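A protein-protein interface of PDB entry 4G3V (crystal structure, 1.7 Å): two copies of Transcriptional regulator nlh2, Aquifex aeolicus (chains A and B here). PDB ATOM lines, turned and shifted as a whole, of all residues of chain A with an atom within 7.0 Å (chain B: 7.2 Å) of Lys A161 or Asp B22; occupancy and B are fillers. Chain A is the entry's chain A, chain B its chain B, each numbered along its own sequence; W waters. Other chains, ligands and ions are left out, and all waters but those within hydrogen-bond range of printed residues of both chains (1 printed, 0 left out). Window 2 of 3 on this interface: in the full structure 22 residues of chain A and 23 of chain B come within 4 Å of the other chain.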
ATOM      1  N   PHE A  25     -15.523 -14.499 -28.051  1.00  0.00           N
ATOM      2  CA  PHE A  25     -14.893 -14.207 -26.768  1.00  0.00           C
ATOM      3  C   PHE A  25     -14.103 -12.903 -26.874  1.00  0.00           C
ATOM      4  O   PHE A  25     -14.298 -11.977 -26.087  1.00  0.00           O
ATOM      5  CB  PHE A  25     -13.976 -15.360 -26.353  1.00  0.00           C
ATOM      6  CG  PHE A  25     -13.342 -15.179 -25.005  1.00  0.00           C
ATOM      7  CD1 PHE A  25     -14.088 -15.308 -23.846  1.00  0.00           C
ATOM      8  CD2 PHE A  25     -11.991 -14.893 -24.895  1.00  0.00           C
ATOM      9  CE1 PHE A  25     -13.491 -15.148 -22.600  1.00  0.00           C
ATOM     10  CE2 PHE A  25     -11.396 -14.733 -23.657  1.00  0.00           C
ATOM     11  CZ  PHE A  25     -12.146 -14.864 -22.508  1.00  0.00           C
ATOM     12  N   LYS A 121     -12.290 -13.521 -11.386  1.00  0.00           N
ATOM     13  CA  LYS A 121     -12.292 -14.792 -10.667  1.00  0.00           C
ATOM     14  C   LYS A 121     -13.413 -15.723 -11.089  1.00  0.00           C
ATOM     15  O   LYS A 121     -14.557 -15.297 -11.260  1.00  0.00           O
ATOM     16  CB  LYS A 121     -12.440 -14.543  -9.175  1.00  0.00           C
ATOM     17  CG  LYS A 121     -11.247 -13.839  -8.551  1.00  0.00           C
ATOM     18  CD  LYS A 121     -11.322 -13.904  -7.031  1.00  0.00           C
ATOM     19  CE  LYS A 121     -10.251 -13.079  -6.395  1.00  0.00           C
ATOM     20  NZ  LYS A 121     -10.299 -13.173  -4.905  1.00  0.00           N
ATOM     21  N   VAL A 122     -13.061 -16.995 -11.222  1.00  0.00           N
ATOM     22  CA  VAL A 122     -14.019 -18.058 -11.472  1.00  0.00           C
ATOM     23  C   VAL A 122     -13.906 -19.082 -10.340  1.00  0.00           C
ATOM     24  O   VAL A 122     -12.836 -19.702 -10.125  1.00  0.00           O
ATOM     25  CB  VAL A 122     -13.742 -18.750 -12.805  1.00  0.00           C
ATOM     26  CG1 VAL A 122     -14.732 -19.883 -13.020  1.00  0.00           C
ATOM     27  CG2 VAL A 122     -13.800 -17.744 -13.951  1.00  0.00           C
ATOM     28  N   GLY A 123     -15.000 -19.261  -9.617  1.00  0.00           N
ATOM     29  CA  GLY A 123     -14.997 -20.128  -8.444  1.00  0.00           C
ATOM     30  C   GLY A 123     -14.022 -19.619  -7.388  1.00  0.00           C
ATOM     31  O   GLY A 123     -13.456 -20.401  -6.618  1.00  0.00           O
ATOM     32  N   LEU A 156     -16.898 -10.074 -15.671  1.00  0.00           N
ATOM     33  CA  LEU A 156     -16.001 -10.803 -16.555  1.00  0.00           C
ATOM     34  C   LEU A 156     -15.738 -12.232 -16.032  1.00  0.00           C
ATOM     35  O   LEU A 156     -15.586 -13.171 -16.814  1.00  0.00           O
ATOM     36  CB  LEU A 156     -14.689 -10.028 -16.736  1.00  0.00           C
ATOM     37  CG  LEU A 156     -14.822  -8.793 -17.634  1.00  0.00           C
ATOM     38  CD1 LEU A 156     -13.612  -7.874 -17.521  1.00  0.00           C
ATOM     39  CD2 LEU A 156     -15.018  -9.215 -19.116  1.00  0.00           C
ATOM     40  N   GLY A 157     -15.675 -12.396 -14.714  1.00  0.00           N
ATOM     41  CA  GLY A 157     -15.525 -13.724 -14.131  1.00  0.00           C
ATOM     42  C   GLY A 157     -16.675 -14.630 -14.558  1.00  0.00           C
ATOM     43  O   GLY A 157     -16.481 -15.775 -14.936  1.00  0.00           O
ATOM     44  N   MET A 158     -17.897 -14.106 -14.510  1.00  0.00           N
ATOM     45  CA  MET A 158     -19.076 -14.848 -14.948  1.00  0.00           C
ATOM     46  C   MET A 158     -18.922 -15.215 -16.420  1.00  0.00           C
ATOM     47  O   MET A 158     -19.216 -16.331 -16.830  1.00  0.00           O
ATOM     48  CB  MET A 158     -20.349 -14.017 -14.774  1.00  0.00           C
ATOM     49  CG  MET A 158     -20.723 -13.666 -13.335  1.00  0.00           C
ATOM     50  SD  MET A 158     -21.265 -15.060 -12.343  1.00  0.00           S
ATOM     51  CE  MET A 158     -22.643 -15.688 -13.289  1.00  0.00           C
ATOM     52  N   PHE A 159     -18.451 -14.251 -17.208  1.00  0.00           N
ATOM     53  CA  PHE A 159     -18.275 -14.454 -18.645  1.00  0.00           C
ATOM     54  C   PHE A 159     -17.247 -15.554 -18.930  1.00  0.00           C
ATOM     55  O   PHE A 159     -17.448 -16.386 -19.828  1.00  0.00           O
ATOM     56  CB  PHE A 159     -17.832 -13.165 -19.320  1.00  0.00           C
ATOM     57  CG  PHE A 159     -17.782 -13.249 -20.830  1.00  0.00           C
ATOM     58  CD1 PHE A 159     -18.935 -13.428 -21.560  1.00  0.00           C
ATOM     59  CD2 PHE A 159     -16.575 -13.145 -21.504  1.00  0.00           C
ATOM     60  CE1 PHE A 159     -18.889 -13.500 -22.950  1.00  0.00           C
ATOM     61  CE2 PHE A 159     -16.515 -13.206 -22.878  1.00  0.00           C
ATOM     62  CZ  PHE A 159     -17.674 -13.385 -23.607  1.00  0.00           C
ATOM     63  N   PHE A 160     -16.143 -15.550 -18.189  1.00  0.00           N
ATOM     64  CA  PHE A 160     -15.128 -16.596 -18.353  1.00  0.00           C
ATOM     65  C   PHE A 160     -15.721 -17.993 -18.087  1.00  0.00           C
ATOM     66  O   PHE A 160     -15.402 -18.974 -18.787  1.00  0.00           O
ATOM     67  CB  PHE A 160     -13.932 -16.369 -17.417  1.00  0.00           C
ATOM     68  CG  PHE A 160     -12.972 -15.283 -17.865  1.00  0.00           C
ATOM     69  CD1 PHE A 160     -13.377 -14.234 -18.679  1.00  0.00           C
ATOM     70  CD2 PHE A 160     -11.649 -15.314 -17.448  1.00  0.00           C
ATOM     71  CE1 PHE A 160     -12.479 -13.241 -19.069  1.00  0.00           C
ATOM     72  CE2 PHE A 160     -10.750 -14.325 -17.822  1.00  0.00           C
ATOM     73  CZ  PHE A 160     -11.161 -13.288 -18.630  1.00  0.00           C
ATOM     74  N   LYS A 161     -16.576 -18.086 -17.074  1.00  0.00           N
ATOM     75  CA  LYS A 161     -17.274 -19.336 -16.763  1.00  0.00           C
ATOM     76  C   LYS A 161     -18.235 -19.705 -17.900  1.00  0.00           C
ATOM     77  O   LYS A 161     -18.298 -20.862 -18.333  1.00  0.00           O
ATOM     78  CB  LYS A 161     -18.041 -19.181 -15.444  1.00  0.00           C
ATOM     79  CG  LYS A 161     -18.832 -20.417 -14.999  1.00  0.00           C
ATOM     80  CD  LYS A 161     -17.936 -21.578 -14.622  1.00  0.00           C
ATOM     81  CE  LYS A 161     -18.760 -22.802 -14.239  1.00  0.00           C
ATOM     82  NZ  LYS A 161     -17.930 -23.882 -13.675  1.00  0.00           N
ATOM     83  N   LEU A 162     -18.964 -18.707 -18.396  1.00  0.00           N
ATOM     84  CA  LEU A 162     -19.910 -18.905 -19.483  1.00  0.00           C
ATOM     85  C   LEU A 162     -19.231 -19.524 -20.703  1.00  0.00           C
ATOM     86  O   LEU A 162     -19.777 -20.426 -21.344  1.00  0.00           O
ATOM     87  CB  LEU A 162     -20.538 -17.568 -19.860  1.00  0.00           C
ATOM     88  CG  LEU A 162     -21.643 -17.580 -20.907  1.00  0.00           C
ATOM     89  CD1 LEU A 162     -22.744 -18.541 -20.517  1.00  0.00           C
ATOM     90  CD2 LEU A 162     -22.193 -16.178 -21.076  1.00  0.00           C
ATOM     91  N   ARG A 163     -18.043 -19.030 -21.013  1.00  0.00           N
ATOM     92  CA  ARG A 163     -17.346 -19.421 -22.232  1.00  0.00           C
ATOM     93  C   ARG A 163     -16.289 -20.495 -21.991  1.00  0.00           C
ATOM     94  O   ARG A 163     -15.476 -20.782 -22.869  1.00  0.00           O
ATOM     95  CB  ARG A 163     -16.731 -18.185 -22.872  1.00  0.00           C
ATOM     96  CG  ARG A 163     -17.776 -17.127 -23.220  1.00  0.00           C
ATOM     97  CD  ARG A 163     -18.805 -17.673 -24.223  1.00  0.00           C
ATOM     98  NE  ARG A 163     -19.716 -16.642 -24.684  1.00  0.00           N
ATOM     99  CZ  ARG A 163     -19.508 -15.865 -25.742  1.00  0.00           C
ATOM    100  NH1 ARG A 163     -18.412 -15.997 -26.485  1.00  0.00           N
ATOM    101  NH2 ARG A 163     -20.404 -14.948 -26.052  1.00  0.00           N
ATOM    102  N   GLU A 164     -16.312 -21.093 -20.806  1.00  0.00           N
ATOM    103  CA  GLU A 164     -15.449 -22.233 -20.503  1.00  0.00           C
ATOM    104  C   GLU A 164     -13.975 -21.903 -20.683  1.00  0.00           C
ATOM    105  O   GLU A 164     -13.254 -22.666 -21.362  1.00  0.00           O
ATOM    106  CB  GLU A 164     -15.763 -23.412 -21.444  1.00  0.00           C
ATOM    107  CG  GLU A 164     -17.176 -23.939 -21.372  1.00  0.00           C
ATOM    108  CD  GLU A 164     -17.340 -25.209 -22.197  1.00  0.00           C
ATOM    109  OE1 GLU A 164     -18.296 -25.977 -21.942  1.00  0.00           O
ATOM    110  OE2 GLU A 164     -16.504 -25.437 -23.102  1.00  0.00           O
ATOM    111  N   LYS B  17     -18.490 -15.874  -6.796  1.00  0.00           N
ATOM    112  CA  LYS B  17     -17.914 -17.182  -6.481  1.00  0.00           C
ATOM    113  C   LYS B  17     -18.986 -18.271  -6.462  1.00  0.00           C
ATOM    114  O   LYS B  17     -18.793 -19.366  -7.008  1.00  0.00           O
ATOM    115  CB  LYS B  17     -17.207 -17.125  -5.134  1.00  0.00           C
ATOM    116  CG  LYS B  17     -16.453 -18.390  -4.759  1.00  0.00           C
ATOM    117  CD  LYS B  17     -15.670 -18.191  -3.473  1.00  0.00           C
ATOM    118  CE  LYS B  17     -14.975 -19.464  -3.030  1.00  0.00           C
ATOM    119  NZ  LYS B  17     -14.302 -19.256  -1.721  1.00  0.00           N
ATOM    120  N   ILE B  18     -20.108 -17.980  -5.820  1.00  0.00           N
ATOM    121  CA  ILE B  18     -21.231 -18.922  -5.764  1.00  0.00           C
ATOM    122  C   ILE B  18     -21.756 -19.233  -7.168  1.00  0.00           C
ATOM    123  O   ILE B  18     -21.898 -20.392  -7.547  1.00  0.00           O
ATOM    124  CB  ILE B  18     -22.382 -18.346  -4.921  1.00  0.00           C
ATOM    125  CG1 ILE B  18     -21.954 -18.250  -3.447  1.00  0.00           C
ATOM    126  CG2 ILE B  18     -23.656 -19.216  -5.058  1.00  0.00           C
ATOM    127  CD1 ILE B  18     -22.806 -17.318  -2.630  1.00  0.00           C
ATOM    128  N   LEU B  19     -22.022 -18.189  -7.943  1.00  0.00           N
ATOM    129  CA  LEU B  19     -22.662 -18.344  -9.253  1.00  0.00           C
ATOM    130  C   LEU B  19     -21.744 -18.884 -10.336  1.00  0.00           C
ATOM    131  O   LEU B  19     -22.222 -19.295 -11.406  1.00  0.00           O
ATOM    132  CB  LEU B  19     -23.275 -17.025  -9.696  1.00  0.00           C
ATOM    133  CG  LEU B  19     -24.357 -16.461  -8.771  1.00  0.00           C
ATOM    134  CD1 LEU B  19     -24.866 -15.135  -9.312  1.00  0.00           C
ATOM    135  CD2 LEU B  19     -25.505 -17.449  -8.591  1.00  0.00           C
ATOM    136  N   THR B  20     -20.438 -18.910 -10.073  1.00  0.00           N
ATOM    137  CA  THR B  20     -19.509 -19.575 -10.988  1.00  0.00           C
ATOM    138  C   THR B  20     -19.090 -20.959 -10.474  1.00  0.00           C
ATOM    139  O   THR B  20     -18.199 -21.607 -11.046  1.00  0.00           O
ATOM    140  CB  THR B  20     -18.258 -18.724 -11.258  1.00  0.00           C
ATOM    141  OG1 THR B  20     -17.584 -18.405 -10.032  1.00  0.00           O
ATOM    142  CG2 THR B  20     -18.651 -17.445 -11.978  1.00  0.00           C
ATOM    143  N   GLY B  21     -19.765 -21.420  -9.425  1.00  0.00           N
ATOM    144  CA  GLY B  21     -19.533 -22.741  -8.869  1.00  0.00           C
ATOM    145  C   GLY B  21     -20.330 -23.802  -9.609  1.00  0.00           C
ATOM    146  O   GLY B  21     -20.680 -23.648 -10.789  1.00  0.00           O
ATOM    147  N   ASP B  22     -20.623 -24.886  -8.919  1.00  0.00           N
ATOM    148  CA  ASP B  22     -21.301 -26.013  -9.537  1.00  0.00           C
ATOM    149  C   ASP B  22     -22.552 -26.430  -8.766  1.00  0.00           C
ATOM    150  O   ASP B  22     -23.030 -27.557  -8.912  1.00  0.00           O
ATOM    151  CB  ASP B  22     -20.333 -27.187  -9.637  1.00  0.00           C
ATOM    152  CG  ASP B  22     -19.165 -26.898 -10.564  1.00  0.00           C
ATOM    153  OD1 ASP B  22     -19.410 -26.779 -11.777  1.00  0.00           O
ATOM    154  OD2 ASP B  22     -18.014 -26.787 -10.092  1.00  0.00           O
ATOM    155  N   TYR B  23     -23.102 -25.519  -7.969  1.00  0.00           N
ATOM    156  CA  TYR B  23     -24.312 -25.823  -7.203  1.00  0.00           C
ATOM    157  C   TYR B  23     -25.511 -25.866  -8.149  1.00  0.00           C
ATOM    158  O   TYR B  23     -25.442 -25.334  -9.264  1.00  0.00           O
ATOM    159  CB  TYR B  23     -24.522 -24.770  -6.101  1.00  0.00           C
ATOM    160  CG  TYR B  23     -23.315 -24.610  -5.200  1.00  0.00           C
ATOM    161  CD1 TYR B  23     -23.017 -25.563  -4.243  1.00  0.00           C
ATOM    162  CD2 TYR B  23     -22.463 -23.514  -5.324  1.00  0.00           C
ATOM    163  CE1 TYR B  23     -21.921 -25.437  -3.440  1.00  0.00           C
ATOM    164  CE2 TYR B  23     -21.356 -23.375  -4.521  1.00  0.00           C
ATOM    165  CZ  TYR B  23     -21.086 -24.339  -3.581  1.00  0.00           C
ATOM    166  OH  TYR B  23     -19.978 -24.223  -2.771  1.00  0.00           O
ATOM    167  N   THR B  24     -26.605 -26.498  -7.729  1.00  0.00           N
ATOM    168  CA  THR B  24     -27.783 -26.552  -8.595  1.00  0.00           C
ATOM    169  C   THR B  24     -28.311 -25.136  -8.760  1.00  0.00           C
ATOM    170  O   THR B  24     -27.927 -24.227  -8.022  1.00  0.00           O
ATOM    171  CB  THR B  24     -28.918 -27.439  -8.042  1.00  0.00           C
ATOM    172  OG1 THR B  24     -29.477 -26.825  -6.880  1.00  0.00           O
ATOM    173  CG2 THR B  24     -28.417 -28.838  -7.696  1.00  0.00           C
ATOM    174  N   PHE B  25     -29.178 -24.948  -9.744  1.00  0.00           N
ATOM    175  CA  PHE B  25     -29.742 -23.633 -10.027  1.00  0.00           C
ATOM    176  C   PHE B  25     -30.441 -23.096  -8.782  1.00  0.00           C
ATOM    177  O   PHE B  25     -30.167 -21.982  -8.334  1.00  0.00           O
ATOM    178  CB  PHE B  25     -30.719 -23.731 -11.202  1.00  0.00           C
ATOM    179  CG  PHE B  25     -31.330 -22.413 -11.594  1.00  0.00           C
ATOM    180  CD1 PHE B  25     -30.593 -21.479 -12.293  1.00  0.00           C
ATOM    181  CD2 PHE B  25     -32.628 -22.108 -11.257  1.00  0.00           C
ATOM    182  CE1 PHE B  25     -31.138 -20.273 -12.661  1.00  0.00           C
ATOM    183  CE2 PHE B  25     -33.188 -20.892 -11.622  1.00  0.00           C
ATOM    184  CZ  PHE B  25     -32.442 -19.974 -12.325  1.00  0.00           C
ATOM    185  N   SER B  28     -28.068 -22.390  -5.788  1.00  0.00           N
ATOM    186  CA  SER B  28     -27.273 -21.175  -6.036  1.00  0.00           C
ATOM    187  C   SER B  28     -28.052 -19.917  -5.681  1.00  0.00           C
ATOM    188  O   SER B  28     -27.543 -19.026  -5.006  1.00  0.00           O
ATOM    189  CB  SER B  28     -26.834 -21.098  -7.499  1.00  0.00           C
ATOM    190  OG  SER B  28     -25.996 -22.195  -7.830  1.00  0.00           O
ATOM    191  N   PHE B 159     -25.910 -15.477 -14.702  1.00  0.00           N
ATOM    192  CA  PHE B 159     -26.119 -16.844 -14.221  1.00  0.00           C
ATOM    193  C   PHE B 159     -27.266 -17.525 -14.975  1.00  0.00           C
ATOM    194  O   PHE B 159     -27.186 -18.712 -15.307  1.00  0.00           O
ATOM    195  CB  PHE B 159     -26.400 -16.824 -12.727  1.00  0.00           C
ATOM    196  CG  PHE B 159     -26.508 -18.196 -12.102  1.00  0.00           C
ATOM    197  CD1 PHE B 159     -25.402 -19.023 -12.009  1.00  0.00           C
ATOM    198  CD2 PHE B 159     -27.718 -18.642 -11.590  1.00  0.00           C
ATOM    199  CE1 PHE B 159     -25.496 -20.276 -11.408  1.00  0.00           C
ATOM    200  CE2 PHE B 159     -27.825 -19.890 -10.990  1.00  0.00           C
ATOM    201  CZ  PHE B 159     -26.712 -20.709 -10.905  1.00  0.00           C
ATOM    202  N   LEU B 162     -25.846 -18.578 -18.168  1.00  0.00           N
ATOM    203  CA  LEU B 162     -24.968 -19.718 -17.941  1.00  0.00           C
ATOM    204  C   LEU B 162     -25.739 -21.034 -17.845  1.00  0.00           C
ATOM    205  O   LEU B 162     -25.314 -22.065 -18.379  1.00  0.00           O
ATOM    206  CB  LEU B 162     -24.202 -19.494 -16.647  1.00  0.00           C
ATOM    207  CG  LEU B 162     -23.256 -20.586 -16.183  1.00  0.00           C
ATOM    208  CD1 LEU B 162     -22.099 -20.762 -17.169  1.00  0.00           C
ATOM    209  CD2 LEU B 162     -22.755 -20.212 -14.808  1.00  0.00           C
ATOM    210  N   ARG B 163     -26.876 -20.999 -17.162  1.00  0.00           N
ATOM    211  CA  ARG B 163     -27.611 -22.223 -16.886  1.00  0.00           C
ATOM    212  C   ARG B 163     -28.750 -22.475 -17.885  1.00  0.00           C
ATOM    213  O   ARG B 163     -29.586 -23.364 -17.686  1.00  0.00           O
ATOM    214  CB  ARG B 163     -28.112 -22.177 -15.456  1.00  0.00           C
ATOM    215  CG  ARG B 163     -26.955 -22.085 -14.445  1.00  0.00           C
ATOM    216  CD  ARG B 163     -26.050 -23.338 -14.504  1.00  0.00           C
ATOM    217  NE  ARG B 163     -25.038 -23.363 -13.444  1.00  0.00           N
ATOM    218  CZ  ARG B 163     -25.237 -23.844 -12.218  1.00  0.00           C
ATOM    219  NH1 ARG B 163     -26.411 -24.358 -11.877  1.00  0.00           N
ATOM    220  NH2 ARG B 163     -24.257 -23.808 -11.326  1.00  0.00           N
HETATM  221  O   HOH W   1     -15.424 -16.165  -8.479  1.00  0.00           O
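The side-chain carboxylate (OD1) of Asp B22 is in salt-bridge range of the side-chain amino group (NZ) of Lys A161 (3.8 Å). The side-chain amino group of Lys A161 sits close to the backbone carbonyl oxygen of Thr B20, at 3.5 Å. The side-chain hydroxyl (OG1) of Thr B20 is in hydrogen-bond range of the backbone NH (N) of Gly A123.
The backbone carbonyl oxygen (O) of Lys B17 is in hydrogen-bond range of the side-chain hydroxyl (OG1) of Thr B20, 3.4 Å away.
Thr B20 touches Val A122. Gly A123 touches Lys B17 (C to CG, 3.8 Å). Leu B19 touches Met A158. Thr B20 touches Met A158. Phe B159 touches Met A158 (N to CE, 3.6 Å). Lys A161 touches Gly B21 (NZ to O, 3.99 Å). Lys A161 touches Leu B162. CD1 of Leu A162 touches CA of Leu B162, at 3.6 Å.
Of the printed residues of chain B, Gly A123 touches Lys B17 (3.8 Å) and Thr B20 (2.8 Å). Leu A156 touches none of the printed residues of chain B. Of the printed residues of chain B, Lys A161 touches Thr B20, Gly B21, Asp B22 and Leu B162. Printed residues of chain A within 4 Å of Leu B19: Met A158. Of the printed residues of chain A, Gly B21 touches Lys A161. The nearest printed residue of chain A that does not touch Asp B22 is Gly A123 (7.4 Å).
Hydrophobic or aromatic side chains of chain A within 4 Å of the printed part of chain B: Met A158 and Leu A162. Along chain A the printed residues that touch a printed residue of chain B span positions 122 to 162. Hydrophobic or aromatic side chains of chain B that line the printed part of chain A: Leu B19, Phe B159 and Leu B162.
Leu A162 touches its own counterpart, Leu B162. Of the 11 pairs that touch across the chains among the printed residues, 1 has its exchanged pair printed and touching as well.
Water W1 lies within hydrogen-bond range of the backbone carbonyl oxygen (O) of Lys A121, the backbone NH (N) of Gly A123 and the side-chain hydroxyl (OG1) of Thr B20.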
